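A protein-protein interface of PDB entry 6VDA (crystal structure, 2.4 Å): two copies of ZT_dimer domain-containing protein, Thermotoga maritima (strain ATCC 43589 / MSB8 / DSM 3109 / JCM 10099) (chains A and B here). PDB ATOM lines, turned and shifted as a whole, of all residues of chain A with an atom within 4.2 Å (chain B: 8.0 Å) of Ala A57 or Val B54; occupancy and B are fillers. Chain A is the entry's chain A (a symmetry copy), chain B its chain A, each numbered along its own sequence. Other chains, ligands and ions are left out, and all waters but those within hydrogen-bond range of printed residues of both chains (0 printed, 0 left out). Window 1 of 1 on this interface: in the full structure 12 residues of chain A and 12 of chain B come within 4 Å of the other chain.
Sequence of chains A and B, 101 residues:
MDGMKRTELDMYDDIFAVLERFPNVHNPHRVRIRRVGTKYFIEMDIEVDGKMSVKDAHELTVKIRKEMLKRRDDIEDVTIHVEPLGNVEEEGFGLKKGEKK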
ATOM      1  N   VAL A  48     -26.976 -31.146   2.870  1.00  0.00           N
ATOM      2  CA  VAL A  48     -26.148 -32.382   2.987  1.00  0.00           C
ATOM      3  C   VAL A  48     -25.111 -32.167   4.086  1.00  0.00           C
ATOM      4  O   VAL A  48     -24.810 -31.005   4.437  1.00  0.00           O
ATOM      5  CB  VAL A  48     -25.490 -32.765   1.649  1.00  0.00           C
ATOM      6  CG1 VAL A  48     -26.532 -32.876   0.544  1.00  0.00           C
ATOM      7  CG2 VAL A  48     -24.374 -31.806   1.250  1.00  0.00           C
ATOM      8  N   GLY A  50     -22.089 -31.243   5.899  1.00  0.00           N
ATOM      9  CA  GLY A  50     -21.072 -30.234   5.554  1.00  0.00           C
ATOM     10  C   GLY A  50     -19.758 -30.874   5.131  1.00  0.00           C
ATOM     11  O   GLY A  50     -18.982 -30.196   4.432  1.00  0.00           O
ATOM     12  N   MET A  52     -19.456 -33.558   3.214  1.00  0.00           N
ATOM     13  CA  MET A  52     -19.607 -34.155   1.857  1.00  0.00           C
ATOM     14  C   MET A  52     -18.771 -33.343   0.862  1.00  0.00           C
ATOM     15  O   MET A  52     -18.786 -32.096   0.944  1.00  0.00           O
ATOM     16  CB  MET A  52     -21.067 -34.177   1.395  1.00  0.00           C
ATOM     17  CG  MET A  52     -21.268 -34.927   0.090  1.00  0.00           C
ATOM     18  SD  MET A  52     -22.971 -34.872  -0.522  1.00  0.00           S
ATOM     19  CE  MET A  52     -23.746 -35.955   0.675  1.00  0.00           C
ATOM     20  N   SER A  53     -18.053 -34.031  -0.025  1.00  0.00           N
ATOM     21  CA  SER A  53     -17.250 -33.412  -1.105  1.00  0.00           C
ATOM     22  C   SER A  53     -18.187 -32.755  -2.125  1.00  0.00           C
ATOM     23  O   SER A  53     -19.366 -33.149  -2.195  1.00  0.00           O
ATOM     24  CB  SER A  53     -16.347 -34.428  -1.744  1.00  0.00           C
ATOM     25  OG  SER A  53     -17.099 -35.391  -2.466  1.00  0.00           O
ATOM     26  N   VAL A  54     -17.671 -31.774  -2.872  1.00  0.00           N
ATOM     27  CA  VAL A  54     -18.363 -31.076  -3.999  1.00  0.00           C
ATOM     28  C   VAL A  54     -18.620 -32.093  -5.124  1.00  0.00           C
ATOM     29  O   VAL A  54     -19.708 -32.034  -5.751  1.00  0.00           O
ATOM     30  CB  VAL A  54     -17.520 -29.868  -4.467  1.00  0.00           C
ATOM     31  CG1 VAL A  54     -17.942 -29.342  -5.826  1.00  0.00           C
ATOM     32  CG2 VAL A  54     -17.529 -28.744  -3.439  1.00  0.00           C
ATOM     33  N   LYS A  55     -17.661 -32.986  -5.384  1.00  0.00           N
ATOM     34  CA  LYS A  55     -17.809 -34.100  -6.359  1.00  0.00           C
ATOM     35  C   LYS A  55     -19.084 -34.881  -6.012  1.00  0.00           C
ATOM     36  O   LYS A  55     -19.957 -35.011  -6.893  1.00  0.00           O
ATOM     37  CB  LYS A  55     -16.573 -35.003  -6.342  1.00  0.00           C
ATOM     38  CG  LYS A  55     -16.485 -36.039  -7.462  1.00  0.00           C
ATOM     39  CD  LYS A  55     -15.887 -35.504  -8.752  1.00  0.00           C
ATOM     40  N   ASP A  56     -19.201 -35.346  -4.767  1.00  0.00           N
ATOM     41  CA  ASP A  56     -20.293 -36.254  -4.324  1.00  0.00           C
ATOM     42  C   ASP A  56     -21.629 -35.516  -4.371  1.00  0.00           C
ATOM     43  O   ASP A  56     -22.592 -36.094  -4.920  1.00  0.00           O
ATOM     44  CB  ASP A  56     -20.010 -36.832  -2.937  1.00  0.00           C
ATOM     45  CG  ASP A  56     -18.941 -37.907  -2.966  1.00  0.00           C
ATOM     46  OD1 ASP A  56     -18.597 -38.353  -4.078  1.00  0.00           O
ATOM     47  OD2 ASP A  56     -18.452 -38.278  -1.881  1.00  0.00           O
ATOM     48  N   ALA A  57     -21.671 -34.302  -3.811  1.00  0.00           N
ATOM     49  CA  ALA A  57     -22.849 -33.406  -3.790  1.00  0.00           C
ATOM     50  C   ALA A  57     -23.323 -33.141  -5.222  1.00  0.00           C
ATOM     51  O   ALA A  57     -24.541 -33.152  -5.454  1.00  0.00           O
ATOM     52  CB  ALA A  57     -22.504 -32.117  -3.086  1.00  0.00           C
ATOM     53  N   HIS A  58     -22.403 -32.906  -6.157  1.00  0.00           N
ATOM     54  CA  HIS A  58     -22.759 -32.616  -7.570  1.00  0.00           C
ATOM     55  C   HIS A  58     -23.374 -33.864  -8.213  1.00  0.00           C
ATOM     56  O   HIS A  58     -24.407 -33.718  -8.917  1.00  0.00           O
ATOM     57  CB  HIS A  58     -21.554 -32.108  -8.368  1.00  0.00           C
ATOM     58  CG  HIS A  58     -21.869 -31.942  -9.815  1.00  0.00           C
ATOM     59  ND1 HIS A  58     -22.466 -30.801 -10.310  1.00  0.00           N
ATOM     60  CD2 HIS A  58     -21.724 -32.786 -10.860  1.00  0.00           C
ATOM     61  CE1 HIS A  58     -22.656 -30.939 -11.607  1.00  0.00           C
ATOM     62  NE2 HIS A  58     -22.212 -32.149 -11.966  1.00  0.00           N
ATOM     63  N   GLU A  59     -22.739 -35.023  -8.012  1.00  0.00           N
ATOM     64  CA  GLU A  59     -23.231 -36.357  -8.456  1.00  0.00           C
ATOM     65  C   GLU A  59     -24.647 -36.587  -7.913  1.00  0.00           C
ATOM     66  O   GLU A  59     -25.490 -37.118  -8.656  1.00  0.00           O
ATOM     67  CB  GLU A  59     -22.307 -37.474  -7.960  1.00  0.00           C
ATOM     68  CG  GLU A  59     -21.203 -37.840  -8.934  1.00  0.00           C
ATOM     69  CD  GLU A  59     -20.176 -38.825  -8.387  1.00  0.00           C
ATOM     70  OE1 GLU A  59     -20.394 -39.371  -7.277  1.00  0.00           O
ATOM     71  OE2 GLU A  59     -19.150 -39.036  -9.067  1.00  0.00           O
ATOM     72  N   LEU A  60     -24.876 -36.222  -6.651  1.00  0.00           N
ATOM     73  CA  LEU A  60     -26.189 -36.365  -5.983  1.00  0.00           C
ATOM     74  C   LEU A  60     -27.241 -35.580  -6.777  1.00  0.00           C
ATOM     75  O   LEU A  60     -28.265 -36.188  -7.139  1.00  0.00           O
ATOM     76  CB  LEU A  60     -26.077 -35.874  -4.537  1.00  0.00           C
ATOM     77  CG  LEU A  60     -27.342 -36.023  -3.695  1.00  0.00           C
ATOM     78  CD1 LEU A  60     -27.850 -37.460  -3.714  1.00  0.00           C
ATOM     79  CD2 LEU A  60     -27.092 -35.561  -2.269  1.00  0.00           C
ATOM     80  N   THR A  61     -26.985 -34.303  -7.079  1.00  0.00           N
ATOM     81  CA  THR A  61     -27.945 -33.425  -7.799  1.00  0.00           C
ATOM     82  C   THR A  61     -28.187 -33.966  -9.216  1.00  0.00           C
ATOM     83  O   THR A  61     -29.330 -33.863  -9.696  1.00  0.00           O
ATOM     84  CB  THR A  61     -27.496 -31.958  -7.808  1.00  0.00           C
ATOM     85  OG1 THR A  61     -26.387 -31.836  -8.695  1.00  0.00           O
ATOM     86  CG2 THR A  61     -27.130 -31.452  -6.430  1.00  0.00           C
ATOM     87  N   VAL A  82     -27.280 -26.723  -3.187  1.00  0.00           N
ATOM     88  CA  VAL A  82     -26.766 -27.583  -2.077  1.00  0.00           C
ATOM     89  C   VAL A  82     -26.233 -26.685  -0.955  1.00  0.00           C
ATOM     90  O   VAL A  82     -25.463 -25.758  -1.254  1.00  0.00           O
ATOM     91  CB  VAL A  82     -25.701 -28.570  -2.586  1.00  0.00           C
ATOM     92  CG1 VAL A  82     -24.954 -29.230  -1.440  1.00  0.00           C
ATOM     93  CG2 VAL A  82     -26.319 -29.617  -3.506  1.00  0.00           C
ATOM     94  N   GLU A  83     -26.653 -26.951   0.285  1.00  0.00           N
ATOM     95  CA  GLU A  83     -26.227 -26.201   1.492  1.00  0.00           C
ATOM     96  C   GLU A  83     -25.745 -27.179   2.555  1.00  0.00           C
ATOM     97  O   GLU A  83     -26.128 -28.350   2.551  1.00  0.00           O
ATOM     98  CB  GLU A  83     -27.381 -25.398   2.088  1.00  0.00           C
ATOM     99  CG  GLU A  83     -28.102 -24.505   1.100  1.00  0.00           C
ATOM    100  CD  GLU A  83     -29.395 -23.948   1.664  1.00  0.00           C
ATOM    101  OE1 GLU A  83     -29.574 -24.013   2.890  1.00  0.00           O
ATOM    102  OE2 GLU A  83     -30.223 -23.452   0.879  1.00  0.00           O
ATOM    103  N   PRO A  84     -24.922 -26.708   3.517  1.00  0.00           N
ATOM    104  CA  PRO A  84     -24.610 -27.481   4.716  1.00  0.00           C
ATOM    105  C   PRO A  84     -25.832 -27.680   5.624  1.00  0.00           C
ATOM    106  O   PRO A  84     -26.689 -26.807   5.661  1.00  0.00           O
ATOM    107  CB  PRO A  84     -23.572 -26.635   5.473  1.00  0.00           C
ATOM    108  CG  PRO A  84     -23.087 -25.616   4.459  1.00  0.00           C
ATOM    109  CD  PRO A  84     -24.251 -25.399   3.512  1.00  0.00           C
ATOM    110  N   VAL B  48     -14.415 -25.518  -8.187  1.00  0.00           N
ATOM    111  CA  VAL B  48     -13.479 -25.750  -7.047  1.00  0.00           C
ATOM    112  C   VAL B  48     -13.025 -27.206  -7.085  1.00  0.00           C
ATOM    113  O   VAL B  48     -13.704 -28.053  -7.705  1.00  0.00           O
ATOM    114  CB  VAL B  48     -14.116 -25.385  -5.694  1.00  0.00           C
ATOM    115  CG1 VAL B  48     -14.652 -23.959  -5.713  1.00  0.00           C
ATOM    116  CG2 VAL B  48     -15.201 -26.368  -5.273  1.00  0.00           C
ATOM    117  N   GLY B  50     -12.826 -30.812  -6.602  1.00  0.00           N
ATOM    118  CA  GLY B  50     -13.905 -31.769  -6.302  1.00  0.00           C
ATOM    119  C   GLY B  50     -13.814 -32.298  -4.879  1.00  0.00           C
ATOM    120  O   GLY B  50     -14.850 -32.760  -4.365  1.00  0.00           O
ATOM    121  N   LYS B  51     -12.627 -32.246  -4.260  1.00  0.00           N
ATOM    122  CA  LYS B  51     -12.380 -32.783  -2.892  1.00  0.00           C
ATOM    123  C   LYS B  51     -12.790 -31.754  -1.827  1.00  0.00           C
ATOM    124  O   LYS B  51     -12.875 -32.144  -0.654  1.00  0.00           O
ATOM    125  CB  LYS B  51     -10.919 -33.217  -2.711  1.00  0.00           C
ATOM    126  CG  LYS B  51     -10.525 -34.509  -3.414  1.00  0.00           C
ATOM    127  N   MET B  52     -13.052 -30.501  -2.203  1.00  0.00           N
ATOM    128  CA  MET B  52     -13.465 -29.434  -1.248  1.00  0.00           C
ATOM    129  C   MET B  52     -14.800 -29.831  -0.608  1.00  0.00           C
ATOM    130  O   MET B  52     -15.689 -30.325  -1.335  1.00  0.00           O
ATOM    131  CB  MET B  52     -13.614 -28.072  -1.933  1.00  0.00           C
ATOM    132  CG  MET B  52     -13.873 -26.939  -0.956  1.00  0.00           C
ATOM    133  SD  MET B  52     -14.156 -25.341  -1.758  1.00  0.00           S
ATOM    134  CE  MET B  52     -12.491 -24.999  -2.321  1.00  0.00           C
ATOM    135  N   SER B  53     -14.919 -29.641   0.705  1.00  0.00           N
ATOM    136  CA  SER B  53     -16.159 -29.897   1.473  1.00  0.00           C
ATOM    137  C   SER B  53     -17.232 -28.880   1.062  1.00  0.00           C
ATOM    138  O   SER B  53     -16.872 -27.805   0.549  1.00  0.00           O
ATOM    139  CB  SER B  53     -15.886 -29.859   2.950  1.00  0.00           C
ATOM    140  OG  SER B  53     -15.556 -28.545   3.371  1.00  0.00           O
ATOM    141  N   VAL B  54     -18.504 -29.231   1.270  1.00  0.00           N
ATOM    142  CA  VAL B  54     -19.698 -28.358   1.053  1.00  0.00           C
ATOM    143  C   VAL B  54     -19.634 -27.181   2.041  1.00  0.00           C
ATOM    144  O   VAL B  54     -19.986 -26.042   1.643  1.00  0.00           O
ATOM    145  CB  VAL B  54     -20.993 -29.191   1.200  1.00  0.00           C
ATOM    146  CG1 VAL B  54     -22.232 -28.334   1.376  1.00  0.00           C
ATOM    147  CG2 VAL B  54     -21.177 -30.154   0.035  1.00  0.00           C
ATOM    148  N   LYS B  55     -19.215 -27.437   3.284  1.00  0.00           N
ATOM    149  CA  LYS B  55     -18.989 -26.386   4.314  1.00  0.00           C
ATOM    150  C   LYS B  55     -18.058 -25.320   3.722  1.00  0.00           C
ATOM    151  O   LYS B  55     -18.450 -24.137   3.702  1.00  0.00           O
ATOM    152  CB  LYS B  55     -18.407 -26.997   5.592  1.00  0.00           C
ATOM    153  CG  LYS B  55     -18.357 -26.077   6.810  1.00  0.00           C
ATOM    154  CD  LYS B  55     -19.650 -26.032   7.604  1.00  0.00           C
ATOM    155  N   ASP B  56     -16.888 -25.731   3.226  1.00  0.00           N
ATOM    156  CA  ASP B  56     -15.815 -24.807   2.770  1.00  0.00           C
ATOM    157  C   ASP B  56     -16.283 -24.044   1.532  1.00  0.00           C
ATOM    158  O   ASP B  56     -16.113 -22.806   1.517  1.00  0.00           O
ATOM    159  CB  ASP B  56     -14.506 -25.555   2.517  1.00  0.00           C
ATOM    160  CG  ASP B  56     -13.809 -25.951   3.804  1.00  0.00           C
ATOM    161  OD1 ASP B  56     -14.223 -25.446   4.866  1.00  0.00           O
ATOM    162  OD2 ASP B  56     -12.870 -26.768   3.736  1.00  0.00           O
ATOM    163  N   ALA B  57     -16.836 -24.763   0.549  1.00  0.00           N
ATOM    164  CA  ALA B  57     -17.392 -24.214  -0.708  1.00  0.00           C
ATOM    165  C   ALA B  57     -18.476 -23.182  -0.386  1.00  0.00           C
ATOM    166  O   ALA B  57     -18.507 -22.132  -1.043  1.00  0.00           O
ATOM    167  CB  ALA B  57     -17.943 -25.332  -1.558  1.00  0.00           C
ATOM    168  N   HIS B  58     -19.344 -23.461   0.587  1.00  0.00           N
ATOM    169  CA  HIS B  58     -20.445 -22.538   0.962  1.00  0.00           C
ATOM    170  C   HIS B  58     -19.861 -21.263   1.583  1.00  0.00           C
ATOM    171  O   HIS B  58     -20.333 -20.157   1.215  1.00  0.00           O
ATOM    172  CB  HIS B  58     -21.456 -23.207   1.898  1.00  0.00           C
ATOM    173  CG  HIS B  58     -22.490 -22.250   2.386  1.00  0.00           C
ATOM    174  ND1 HIS B  58     -23.620 -21.954   1.650  1.00  0.00           N
ATOM    175  CD2 HIS B  58     -22.541 -21.484   3.496  1.00  0.00           C
ATOM    176  CE1 HIS B  58     -24.337 -21.061   2.301  1.00  0.00           C
ATOM    177  NE2 HIS B  58     -23.694 -20.755   3.434  1.00  0.00           N
ATOM    178  N   GLU B  59     -18.912 -21.424   2.510  1.00  0.00           N
ATOM    179  CA  GLU B  59     -18.144 -20.318   3.150  1.00  0.00           C
ATOM    180  C   GLU B  59     -17.491 -19.455   2.065  1.00  0.00           C
ATOM    181  O   GLU B  59     -17.493 -18.220   2.206  1.00  0.00           O
ATOM    182  CB  GLU B  59     -17.063 -20.872   4.083  1.00  0.00           C
ATOM    183  CG  GLU B  59     -17.517 -21.047   5.520  1.00  0.00           C
ATOM    184  CD  GLU B  59     -16.511 -21.754   6.421  1.00  0.00           C
ATOM    185  OE1 GLU B  59     -15.360 -21.986   5.976  1.00  0.00           O
ATOM    186  OE2 GLU B  59     -16.885 -22.086   7.565  1.00  0.00           O
ATOM    187  N   LEU B  60     -16.928 -20.096   1.040  1.00  0.00           N
ATOM    188  CA  LEU B  60     -16.268 -19.410  -0.093  1.00  0.00           C
ATOM    189  C   LEU B  60     -17.280 -18.477  -0.769  1.00  0.00           C
ATOM    190  O   LEU B  60     -16.962 -17.282  -0.909  1.00  0.00           O
ATOM    191  CB  LEU B  60     -15.714 -20.456  -1.064  1.00  0.00           C
ATOM    192  CG  LEU B  60     -14.941 -19.897  -2.257  1.00  0.00           C
ATOM    193  CD1 LEU B  60     -13.820 -18.971  -1.801  1.00  0.00           C
ATOM    194  CD2 LEU B  60     -14.391 -21.026  -3.112  1.00  0.00           C
ATOM    195  N   THR B  61     -18.466 -18.980  -1.129  1.00  0.00           N
ATOM    196  CA  THR B  61     -19.509 -18.191  -1.836  1.00  0.00           C
ATOM    197  C   THR B  61     -19.995 -17.043  -0.937  1.00  0.00           C
ATOM    198  O   THR B  61     -20.279 -15.958  -1.475  1.00  0.00           O
ATOM    199  CB  THR B  61     -20.666 -19.068  -2.330  1.00  0.00           C
ATOM    200  OG1 THR B  61     -21.433 -19.474  -1.201  1.00  0.00           O
ATOM    201  CG2 THR B  61     -20.191 -20.275  -3.109  1.00  0.00           C
ATOM    202  N   VAL B  82     -21.655 -23.659  -7.503  1.00  0.00           N
ATOM    203  CA  VAL B  82     -20.333 -24.328  -7.305  1.00  0.00           C
ATOM    204  C   VAL B  82     -20.335 -25.668  -8.048  1.00  0.00           C
ATOM    205  O   VAL B  82     -21.300 -26.433  -7.888  1.00  0.00           O
ATOM    206  CB  VAL B  82     -20.012 -24.494  -5.809  1.00  0.00           C
ATOM    207  CG1 VAL B  82     -18.839 -25.433  -5.587  1.00  0.00           C
ATOM    208  CG2 VAL B  82     -19.760 -23.143  -5.149  1.00  0.00           C
ATOM    209  N   PRO B  84     -17.542 -29.062  -9.598  1.00  0.00           N
ATOM    210  CA  PRO B  84     -16.209 -29.658  -9.625  1.00  0.00           C
ATOM    211  C   PRO B  84     -15.359 -29.150 -10.799  1.00  0.00           C
ATOM    212  O   PRO B  84     -15.918 -28.844 -11.844  1.00  0.00           O
ATOM    213  CB  PRO B  84     -16.454 -31.164  -9.817  1.00  0.00           C
ATOM    214  CG  PRO B  84     -17.925 -31.363  -9.506  1.00  0.00           C
ATOM    215  CD  PRO B  84     -18.596 -30.052  -9.866  1.00  0.00           C
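Of chain B, only Val B54 (3.9 Å) comes within 4 Å of Ala A57.
Of the printed residues of chain A, Val B54 touches Val A48, Gly A50, Met A52, Ala A57, Glu A83 and Pro A84.
Of the printed residues of chain A, Met B52 touches Ser A53 (3.5 Å) and Val A54 (2.9 Å).
Of the printed residues of chain B, His A58 touches Pro B84.
Printed residues of chain A within 4 Å of Ala B57: Val A54.
Of the printed residues of chain A, Val B48 touches Val A54.
The nearest printed residue of chain A that does not touch Val B54 is Val A82 (4.02 Å).
SD of Met B52 lies within hydrogen-bond range of N of Ala B57, at 3.6 Å.
The side-chain hydroxyl of Ser B53 is in hydrogen-bond range of the backbone NH of Asp B56 (3.1 Å).
O of His B58 sits at hydrogen-bond distance from OG1 of Thr B61, at 2.7 Å.
The backbone NH of Val A48 sits at hydrogen-bond distance from the backbone carbonyl oxygen of Glu A83 (2.9 Å).
The backbone NH (N) of Ala A57 lies within hydrogen-bond range of the side-chain sulfur (SD) of Met A52 (3.6 Å).
The side-chain hydroxyl of Thr A61 sits at hydrogen-bond distance from the backbone carbonyl oxygen of His A58 (2.7 Å).
Of the 15 printed residues of chain B, 9 touch a printed residue of chain A.
Hydrophobic or aromatic side chains of chain A within 4 Å of the printed part of chain B: Val A48, Val A54, Ala A57, His A58 and Pro A84.
The backbone NH (N) of Val A54 sits at hydrogen-bond distance from the backbone carbonyl oxygen (O) of Gly B50.
The backbone NH (N) of Lys A55 lies within hydrogen-bond range of the backbone carbonyl oxygen (O) of Gly B50.
O of Met B52 sits at hydrogen-bond distance from N of Val A54 (2.9 Å).
The backbone NH of Val B54 lies within hydrogen-bond range of the backbone carbonyl oxygen of Gly A50, at 3.3 Å.
N of Val B54 lies within hydrogen-bond range of O of Met A52 (2.9 Å).
N of Lys B55 is in hydrogen-bond range of O of Gly A50, at 3.0 Å.
Among the printed residues, pairs that only touch across the chains: Val A48 with Val B54 (3.8 Å), Gly A50 with Ser B53 (3.4 Å), Met A52 with Ser B53 (3.5 Å), Ser A53 with Gly B50 (3.4 Å), Ser A53 with Met B52 (3.5 Å), Val A54 with Val B48 (3.8 Å), Val A54 with Ala B57 (3.9 Å), Val A54 with Pro B84 (3.8 Å), Ala A57 with Val B54 (3.9 Å), His A58 with Pro B84 (3.8 Å), Glu A83 with Val B54 (3.9 Å), Pro A84 with Val B54 (3.8 Å) and Pro A84 with His B58 (3.8 Å).
Val A48 touches Val B54, and with the chains exchanged Val A54 touches Val B48.
Gly A50 touches Lys B55, and with the chains exchanged Lys A55 touches Gly B50.
Met A52 touches Ser B53, and with the chains exchanged Ser A53 touches Met B52.
Met A52 touches Val B54, and with the chains exchanged Val A54 touches Met B52.
14 positions are printed for both chains.
Of the 19 pairs that touch across the chains among the printed residues, 18 have their exchanged pair printed and touching as well.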
